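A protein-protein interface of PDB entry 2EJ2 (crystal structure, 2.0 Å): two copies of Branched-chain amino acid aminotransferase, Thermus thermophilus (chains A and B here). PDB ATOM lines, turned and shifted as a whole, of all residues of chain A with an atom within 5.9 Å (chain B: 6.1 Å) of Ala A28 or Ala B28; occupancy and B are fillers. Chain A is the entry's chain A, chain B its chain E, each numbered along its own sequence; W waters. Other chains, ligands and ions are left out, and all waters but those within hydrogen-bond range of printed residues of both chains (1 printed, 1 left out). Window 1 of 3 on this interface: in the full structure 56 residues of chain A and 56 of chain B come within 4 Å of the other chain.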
ATOM      1  N   SER A  26      -1.726  11.022  -5.151  1.00  0.00           N
ATOM      2  CA  SER A  26      -1.013   9.757  -5.323  1.00  0.00           C
ATOM      3  C   SER A  26      -0.212   9.781  -6.621  1.00  0.00           C
ATOM      4  O   SER A  26      -0.727  10.141  -7.681  1.00  0.00           O
ATOM      5  CB  SER A  26      -1.990   8.578  -5.354  1.00  0.00           C
ATOM      6  OG  SER A  26      -2.660   8.432  -4.117  1.00  0.00           O
ATOM      7  N   HIS A  27       1.052   9.392  -6.521  1.00  0.00           N
ATOM      8  CA  HIS A  27       1.970   9.363  -7.655  1.00  0.00           C
ATOM      9  C   HIS A  27       1.345   8.703  -8.895  1.00  0.00           C
ATOM     10  O   HIS A  27       1.397   9.251  -9.996  1.00  0.00           O
ATOM     11  CB  HIS A  27       3.241   8.626  -7.218  1.00  0.00           C
ATOM     12  CG  HIS A  27       4.428   8.847  -8.106  1.00  0.00           C
ATOM     13  ND1 HIS A  27       4.649   8.118  -9.254  1.00  0.00           N
ATOM     14  CD2 HIS A  27       5.481   9.692  -7.989  1.00  0.00           C
ATOM     15  CE1 HIS A  27       5.788   8.501  -9.806  1.00  0.00           C
ATOM     16  NE2 HIS A  27       6.312   9.456  -9.058  1.00  0.00           N
ATOM     17  N   ALA A  28       0.728   7.542  -8.708  1.00  0.00           N
ATOM     18  CA  ALA A  28       0.125   6.801  -9.815  1.00  0.00           C
ATOM     19  C   ALA A  28      -0.995   7.530 -10.552  1.00  0.00           C
ATOM     20  O   ALA A  28      -1.207   7.306 -11.744  1.00  0.00           O
ATOM     21  CB  ALA A  28      -0.377   5.452  -9.317  1.00  0.00           C
ATOM     22  N   LEU A  29      -1.714   8.397  -9.848  1.00  0.00           N
ATOM     23  CA  LEU A  29      -2.808   9.133 -10.464  1.00  0.00           C
ATOM     24  C   LEU A  29      -2.246  10.201 -11.398  1.00  0.00           C
ATOM     25  O   LEU A  29      -2.917  10.648 -12.331  1.00  0.00           O
ATOM     26  CB  LEU A  29      -3.672   9.790  -9.379  1.00  0.00           C
ATOM     27  CG  LEU A  29      -5.050  10.292  -9.818  1.00  0.00           C
ATOM     28  CD1 LEU A  29      -5.902   9.107 -10.266  1.00  0.00           C
ATOM     29  CD2 LEU A  29      -5.726  11.022  -8.659  1.00  0.00           C
ATOM     30  N   HIS A  30      -1.002  10.596 -11.147  1.00  0.00           N
ATOM     31  CA  HIS A  30      -0.342  11.620 -11.947  1.00  0.00           C
ATOM     32  C   HIS A  30       0.642  11.078 -12.983  1.00  0.00           C
ATOM     33  O   HIS A  30       0.801  11.663 -14.051  1.00  0.00           O
ATOM     34  CB  HIS A  30       0.443  12.583 -11.042  1.00  0.00           C
ATOM     35  CG  HIS A  30      -0.406  13.380 -10.102  1.00  0.00           C
ATOM     36  ND1 HIS A  30      -0.394  14.759 -10.079  1.00  0.00           N
ATOM     37  CD2 HIS A  30      -1.273  12.995  -9.135  1.00  0.00           C
ATOM     38  CE1 HIS A  30      -1.219  15.187  -9.139  1.00  0.00           C
ATOM     39  NE2 HIS A  30      -1.765  14.138  -8.552  1.00  0.00           N
ATOM     40  N   TYR A  31       1.298   9.966 -12.673  1.00  0.00           N
ATOM     41  CA  TYR A  31       2.317   9.445 -13.572  1.00  0.00           C
ATOM     42  C   TYR A  31       2.170   8.015 -14.087  1.00  0.00           C
ATOM     43  O   TYR A  31       3.139   7.445 -14.598  1.00  0.00           O
ATOM     44  CB  TYR A  31       3.680   9.607 -12.895  1.00  0.00           C
ATOM     45  CG  TYR A  31       3.940  11.006 -12.351  1.00  0.00           C
ATOM     46  CD1 TYR A  31       4.257  11.203 -11.006  1.00  0.00           C
ATOM     47  CD2 TYR A  31       3.908  12.121 -13.185  1.00  0.00           C
ATOM     48  CE1 TYR A  31       4.544  12.479 -10.502  1.00  0.00           C
ATOM     49  CE2 TYR A  31       4.194  13.407 -12.692  1.00  0.00           C
ATOM     50  CZ  TYR A  31       4.513  13.575 -11.350  1.00  0.00           C
ATOM     51  OH  TYR A  31       4.816  14.830 -10.859  1.00  0.00           O
ATOM     52  N   GLY A  32       0.973   7.444 -13.957  1.00  0.00           N
ATOM     53  CA  GLY A  32       0.723   6.093 -14.437  1.00  0.00           C
ATOM     54  C   GLY A  32       1.525   4.996 -13.756  1.00  0.00           C
ATOM     55  O   GLY A  32       1.625   3.875 -14.262  1.00  0.00           O
ATOM     56  N   THR A  33       2.073   5.308 -12.589  1.00  0.00           N
ATOM     57  CA  THR A  33       2.891   4.362 -11.845  1.00  0.00           C
ATOM     58  C   THR A  33       2.133   3.345 -10.988  1.00  0.00           C
ATOM     59  O   THR A  33       2.193   3.374  -9.757  1.00  0.00           O
ATOM     60  CB  THR A  33       3.897   5.124 -10.966  1.00  0.00           C
ATOM     61  OG1 THR A  33       3.221   6.189 -10.279  1.00  0.00           O
ATOM     62  CG2 THR A  33       5.006   5.708 -11.832  1.00  0.00           C
ATOM     63  N   SER A  34       1.433   2.435 -11.656  1.00  0.00           N
ATOM     64  CA  SER A  34       0.686   1.384 -10.984  1.00  0.00           C
ATOM     65  C   SER A  34       0.805   0.114 -11.809  1.00  0.00           C
ATOM     66  O   SER A  34       1.194   0.161 -12.974  1.00  0.00           O
ATOM     67  CB  SER A  34      -0.795   1.760 -10.862  1.00  0.00           C
ATOM     68  OG  SER A  34      -1.413   1.837 -12.141  1.00  0.00           O
ATOM     69  N   TRP A 101      -0.335   0.569  -6.372  1.00  0.00           N
ATOM     70  CA  TRP A 101       0.005   1.879  -6.904  1.00  0.00           C
ATOM     71  C   TRP A 101       0.906   2.703  -5.990  1.00  0.00           C
ATOM     72  O   TRP A 101       0.916   2.505  -4.772  1.00  0.00           O
ATOM     73  CB  TRP A 101      -1.284   2.654  -7.222  1.00  0.00           C
ATOM     74  CG  TRP A 101      -2.058   3.119  -6.014  1.00  0.00           C
ATOM     75  CD1 TRP A 101      -2.036   4.369  -5.458  1.00  0.00           C
ATOM     76  CD2 TRP A 101      -2.973   2.344  -5.224  1.00  0.00           C
ATOM     77  NE1 TRP A 101      -2.884   4.422  -4.374  1.00  0.00           N
ATOM     78  CE2 TRP A 101      -3.470   3.193  -4.208  1.00  0.00           C
ATOM     79  CE3 TRP A 101      -3.418   1.017  -5.276  1.00  0.00           C
ATOM     80  CZ2 TRP A 101      -4.394   2.756  -3.251  1.00  0.00           C
ATOM     81  CZ3 TRP A 101      -4.338   0.581  -4.321  1.00  0.00           C
ATOM     82  CH2 TRP A 101      -4.815   1.451  -3.323  1.00  0.00           C
ATOM     83  N   MET A 102       1.675   3.608  -6.592  1.00  0.00           N
ATOM     84  CA  MET A 102       2.561   4.482  -5.834  1.00  0.00           C
ATOM     85  C   MET A 102       1.695   5.577  -5.211  1.00  0.00           C
ATOM     86  O   MET A 102       0.903   6.222  -5.904  1.00  0.00           O
ATOM     87  CB  MET A 102       3.631   5.086  -6.748  1.00  0.00           C
ATOM     88  CG  MET A 102       4.558   4.048  -7.381  1.00  0.00           C
ATOM     89  SD  MET A 102       5.202   2.856  -6.168  1.00  0.00           S
ATOM     90  CE  MET A 102       6.295   3.891  -5.241  1.00  0.00           C
ATOM     91  N   GLY A 103       1.859   5.768  -3.902  1.00  0.00           N
ATOM     92  CA  GLY A 103       1.069   6.733  -3.154  1.00  0.00           C
ATOM     93  C   GLY A 103       1.425   8.208  -3.172  1.00  0.00           C
ATOM     94  O   GLY A 103       2.159   8.685  -4.038  1.00  0.00           O
ATOM     95  N   LEU B  25     -10.948   2.736  -7.804  1.00  0.00           N
ATOM     96  CA  LEU B  25     -11.455   2.105  -9.020  1.00  0.00           C
ATOM     97  C   LEU B  25     -11.457   3.126 -10.150  1.00  0.00           C
ATOM     98  O   LEU B  25     -12.001   2.878 -11.224  1.00  0.00           O
ATOM     99  CB  LEU B  25     -12.879   1.568  -8.816  1.00  0.00           C
ATOM    100  CG  LEU B  25     -13.078   0.454  -7.788  1.00  0.00           C
ATOM    101  CD1 LEU B  25     -14.554   0.062  -7.749  1.00  0.00           C
ATOM    102  CD2 LEU B  25     -12.214  -0.749  -8.143  1.00  0.00           C
ATOM    103  N   SER B  26     -10.853   4.284  -9.897  1.00  0.00           N
ATOM    104  CA  SER B  26     -10.772   5.333 -10.908  1.00  0.00           C
ATOM    105  C   SER B  26      -9.954   4.833 -12.095  1.00  0.00           C
ATOM    106  O   SER B  26      -8.880   4.252 -11.929  1.00  0.00           O
ATOM    107  CB  SER B  26     -10.119   6.590 -10.332  1.00  0.00           C
ATOM    108  OG  SER B  26     -10.919   7.159  -9.311  1.00  0.00           O
ATOM    109  N   HIS B  27     -10.481   5.066 -13.289  1.00  0.00           N
ATOM    110  CA  HIS B  27      -9.853   4.651 -14.532  1.00  0.00           C
ATOM    111  C   HIS B  27      -8.386   5.106 -14.626  1.00  0.00           C
ATOM    112  O   HIS B  27      -7.518   4.333 -15.032  1.00  0.00           O
ATOM    113  CB  HIS B  27     -10.679   5.214 -15.691  1.00  0.00           C
ATOM    114  CG  HIS B  27     -10.420   4.560 -17.013  1.00  0.00           C
ATOM    115  ND1 HIS B  27      -9.359   4.908 -17.823  1.00  0.00           N
ATOM    116  CD2 HIS B  27     -11.120   3.620 -17.692  1.00  0.00           C
ATOM    117  CE1 HIS B  27      -9.422   4.214 -18.946  1.00  0.00           C
ATOM    118  NE2 HIS B  27     -10.481   3.425 -18.892  1.00  0.00           N
ATOM    119  N   ALA B  28      -8.114   6.347 -14.226  1.00  0.00           N
ATOM    120  CA  ALA B  28      -6.755   6.897 -14.276  1.00  0.00           C
ATOM    121  C   ALA B  28      -5.742   6.196 -13.367  1.00  0.00           C
ATOM    122  O   ALA B  28      -4.539   6.223 -13.635  1.00  0.00           O
ATOM    123  CB  ALA B  28      -6.787   8.390 -13.957  1.00  0.00           C
ATOM    124  N   LEU B  29      -6.218   5.579 -12.290  1.00  0.00           N
ATOM    125  CA  LEU B  29      -5.326   4.887 -11.373  1.00  0.00           C
ATOM    126  C   LEU B  29      -4.926   3.534 -11.967  1.00  0.00           C
ATOM    127  O   LEU B  29      -3.913   2.949 -11.586  1.00  0.00           O
ATOM    128  CB  LEU B  29      -6.014   4.674 -10.016  1.00  0.00           C
ATOM    129  CG  LEU B  29      -5.092   4.353  -8.829  1.00  0.00           C
ATOM    130  CD1 LEU B  29      -4.173   5.551  -8.570  1.00  0.00           C
ATOM    131  CD2 LEU B  29      -5.913   4.037  -7.578  1.00  0.00           C
ATOM    132  N   HIS B  30      -5.729   3.045 -12.907  1.00  0.00           N
ATOM    133  CA  HIS B  30      -5.471   1.756 -13.543  1.00  0.00           C
ATOM    134  C   HIS B  30      -4.828   1.836 -14.920  1.00  0.00           C
ATOM    135  O   HIS B  30      -4.009   0.982 -15.278  1.00  0.00           O
ATOM    136  CB  HIS B  30      -6.779   0.968 -13.693  1.00  0.00           C
ATOM    137  CG  HIS B  30      -7.404   0.570 -12.392  1.00  0.00           C
ATOM    138  ND1 HIS B  30      -7.484  -0.742 -11.977  1.00  0.00           N
ATOM    139  CD2 HIS B  30      -7.982   1.309 -11.417  1.00  0.00           C
ATOM    140  CE1 HIS B  30      -8.086  -0.794 -10.802  1.00  0.00           C
ATOM    141  NE2 HIS B  30      -8.398   0.438 -10.440  1.00  0.00           N
ATOM    142  N   TYR B  31      -5.196   2.865 -15.680  1.00  0.00           N
ATOM    143  CA  TYR B  31      -4.733   3.010 -17.052  1.00  0.00           C
ATOM    144  C   TYR B  31      -3.983   4.290 -17.458  1.00  0.00           C
ATOM    145  O   TYR B  31      -3.838   4.560 -18.649  1.00  0.00           O
ATOM    146  CB  TYR B  31      -5.940   2.820 -17.978  1.00  0.00           C
ATOM    147  CG  TYR B  31      -6.773   1.587 -17.660  1.00  0.00           C
ATOM    148  CD1 TYR B  31      -8.121   1.704 -17.309  1.00  0.00           C
ATOM    149  CD2 TYR B  31      -6.219   0.306 -17.723  1.00  0.00           C
ATOM    150  CE1 TYR B  31      -8.899   0.579 -17.030  1.00  0.00           C
ATOM    151  CE2 TYR B  31      -6.987  -0.829 -17.447  1.00  0.00           C
ATOM    152  CZ  TYR B  31      -8.326  -0.685 -17.101  1.00  0.00           C
ATOM    153  OH  TYR B  31      -9.092  -1.800 -16.826  1.00  0.00           O
ATOM    154  N   GLY B  32      -3.524   5.070 -16.481  1.00  0.00           N
ATOM    155  CA  GLY B  32      -2.774   6.288 -16.766  1.00  0.00           C
ATOM    156  C   GLY B  32      -3.524   7.378 -17.504  1.00  0.00           C
ATOM    157  O   GLY B  32      -2.917   8.308 -18.050  1.00  0.00           O
ATOM    158  N   THR B  33      -4.848   7.281 -17.508  1.00  0.00           N
ATOM    159  CA  THR B  33      -5.682   8.250 -18.203  1.00  0.00           C
ATOM    160  C   THR B  33      -5.980   9.546 -17.444  1.00  0.00           C
ATOM    161  O   THR B  33      -7.120   9.809 -17.039  1.00  0.00           O
ATOM    162  CB  THR B  33      -7.007   7.605 -18.625  1.00  0.00           C
ATOM    163  OG1 THR B  33      -7.594   6.952 -17.494  1.00  0.00           O
ATOM    164  CG2 THR B  33      -6.765   6.581 -19.733  1.00  0.00           C
ATOM    165  N   SER B  34      -4.946  10.358 -17.258  1.00  0.00           N
ATOM    166  CA  SER B  34      -5.094  11.645 -16.594  1.00  0.00           C
ATOM    167  C   SER B  34      -4.214  12.647 -17.319  1.00  0.00           C
ATOM    168  O   SER B  34      -3.356  12.265 -18.120  1.00  0.00           O
ATOM    169  CB  SER B  34      -4.655  11.557 -15.132  1.00  0.00           C
ATOM    170  OG  SER B  34      -3.267  11.284 -15.030  1.00  0.00           O
ATOM    171  N   ALA B 100      -6.642  16.501 -14.008  1.00  0.00           N
ATOM    172  CA  ALA B 100      -7.938  16.058 -14.513  1.00  0.00           C
ATOM    173  C   ALA B 100      -7.743  14.568 -14.768  1.00  0.00           C
ATOM    174  O   ALA B 100      -6.766  14.172 -15.415  1.00  0.00           O
ATOM    175  CB  ALA B 100      -8.282  16.781 -15.805  1.00  0.00           C
ATOM    176  N   TRP B 101      -8.645  13.739 -14.249  1.00  0.00           N
ATOM    177  CA  TRP B 101      -8.508  12.299 -14.419  1.00  0.00           C
ATOM    178  C   TRP B 101      -9.836  11.583 -14.639  1.00  0.00           C
ATOM    179  O   TRP B 101     -10.895  12.055 -14.208  1.00  0.00           O
ATOM    180  CB  TRP B 101      -7.792  11.703 -13.201  1.00  0.00           C
ATOM    181  CG  TRP B 101      -8.616  11.671 -11.933  1.00  0.00           C
ATOM    182  CD1 TRP B 101      -9.344  10.618 -11.457  1.00  0.00           C
ATOM    183  CD2 TRP B 101      -8.783  12.734 -10.985  1.00  0.00           C
ATOM    184  NE1 TRP B 101      -9.951  10.955 -10.272  1.00  0.00           N
ATOM    185  CE2 TRP B 101      -9.625  12.249  -9.959  1.00  0.00           C
ATOM    186  CE3 TRP B 101      -8.304  14.049 -10.901  1.00  0.00           C
ATOM    187  CZ2 TRP B 101     -10.000  13.037  -8.858  1.00  0.00           C
ATOM    188  CZ3 TRP B 101      -8.677  14.833  -9.806  1.00  0.00           C
ATOM    189  CH2 TRP B 101      -9.517  14.321  -8.800  1.00  0.00           C
ATOM    190  N   MET B 102      -9.773  10.441 -15.319  1.00  0.00           N
ATOM    191  CA  MET B 102     -10.967   9.650 -15.582  1.00  0.00           C
ATOM    192  C   MET B 102     -11.322   8.915 -14.298  1.00  0.00           C
ATOM    193  O   MET B 102     -10.460   8.291 -13.676  1.00  0.00           O
ATOM    194  CB  MET B 102     -10.711   8.661 -16.722  1.00  0.00           C
ATOM    195  CG  MET B 102     -10.367   9.330 -18.047  1.00  0.00           C
ATOM    196  SD  MET B 102     -11.500  10.682 -18.485  1.00  0.00           S
ATOM    197  CE  MET B 102     -12.964   9.792 -18.895  1.00  0.00           C
ATOM    198  N   GLY B 103     -12.595   8.996 -13.910  1.00  0.00           N
ATOM    199  CA  GLY B 103     -13.060   8.381 -12.677  1.00  0.00           C
ATOM    200  C   GLY B 103     -13.449   6.913 -12.674  1.00  0.00           C
ATOM    201  O   GLY B 103     -13.091   6.154 -13.573  1.00  0.00           O
HETATM  202  O   HOH W   1      -2.205   4.533 -13.763  1.00  0.00           O
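Among the printed residues, pairs that only touch across the chains: Ala A28 with Ala B28 (3.98 Å), Ala A28 with Leu B29 (3.9 Å), Leu A29 with Ala B28 (3.9 Å), Leu A29 with Leu B29 (3.97 Å), Leu A29 with Trp B101 (3.9 Å) and Trp A101 with Leu B29 (3.96 Å).
Water W1 lies within hydrogen-bond range of the backbone carbonyl oxygen of Ala B28, the backbone NH of Gly B32, the backbone carbonyl oxygen of Leu B29 and the side-chain hydroxyl of Ser A34.
The backbone carbonyl oxygen of Leu A29 is in hydrogen-bond range of the side-chain hydroxyl of Ser B34, at 2.8 Å.
The side-chain hydroxyl (OG) of Ser A34 lies within hydrogen-bond range of the backbone carbonyl oxygen (O) of Leu B29 (2.8 Å).
The backbone carbonyl oxygen (O) of Met B102 lies within hydrogen-bond range of the backbone NH (N) of Ala B28 (3.1 Å).
The side-chain hydroxyl of Thr A33 lies close to the backbone NH of Ala A28 (3.2 Å).
O of Met A102 sits at hydrogen-bond distance from N of Ala A28, at 3.1 Å.
N of Ala B28 lies close to OG1 of Thr B33 (3.4 Å).
Ala B28 touches its own counterpart, Ala A28.
Ala A28 touches Leu B29, and with the chains exchanged Leu A29 touches Ala B28.
Leu A29 touches its own counterpart, Leu B29.
Leu A29 touches Trp B101, and with the chains exchanged Trp A101 touches Leu B29.
12 positions are printed for both chains.
Of the 8 pairs that touch across the chains among the printed residues, 8 have their exchanged pair printed and touching as well.
Printed residues of chain B that touch a printed residue of chain A: Ala B28, Leu B29, Ser B34 and Trp B101.
Hydrophobic or aromatic side chains of chain B within 4 Å of the printed part of chain A: Ala B28, Leu B29 and Trp B101.
Along chain B the printed residues that touch a printed residue of chain A span positions 28 to 101.
Hydrophobic or aromatic side chains of chain A within 4 Å of the printed part of chain B: Ala A28, Leu A29 and Trp A101.
Among the printed residues, 8 pairs touch across the chains.
Printed residues of chain B within 4 Å of Ala A28: Ala B28 and Leu B29.
Of the printed residues of chain A, Ala B28 touches Ala A28 (3.98 Å) and Leu A29 (3.9 Å).
Of the printed residues of chain A, Ser B34 touches Leu A29.
Of the printed residues of chain B, Ser A34 touches Leu B29 (2.8 Å).
Gly B103 touches none of the printed residues of chain A.
The nearest printed residue of chain B that does not touch Ala A28 is Gly B32 (5.4 Å).
The nearest printed residue of chain A that does not touch Ala B28 is Gly A32 (5.3 Å).
The nearest printed residue of chain B that does not touch Ser A34 is His B30 (4.2 Å).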
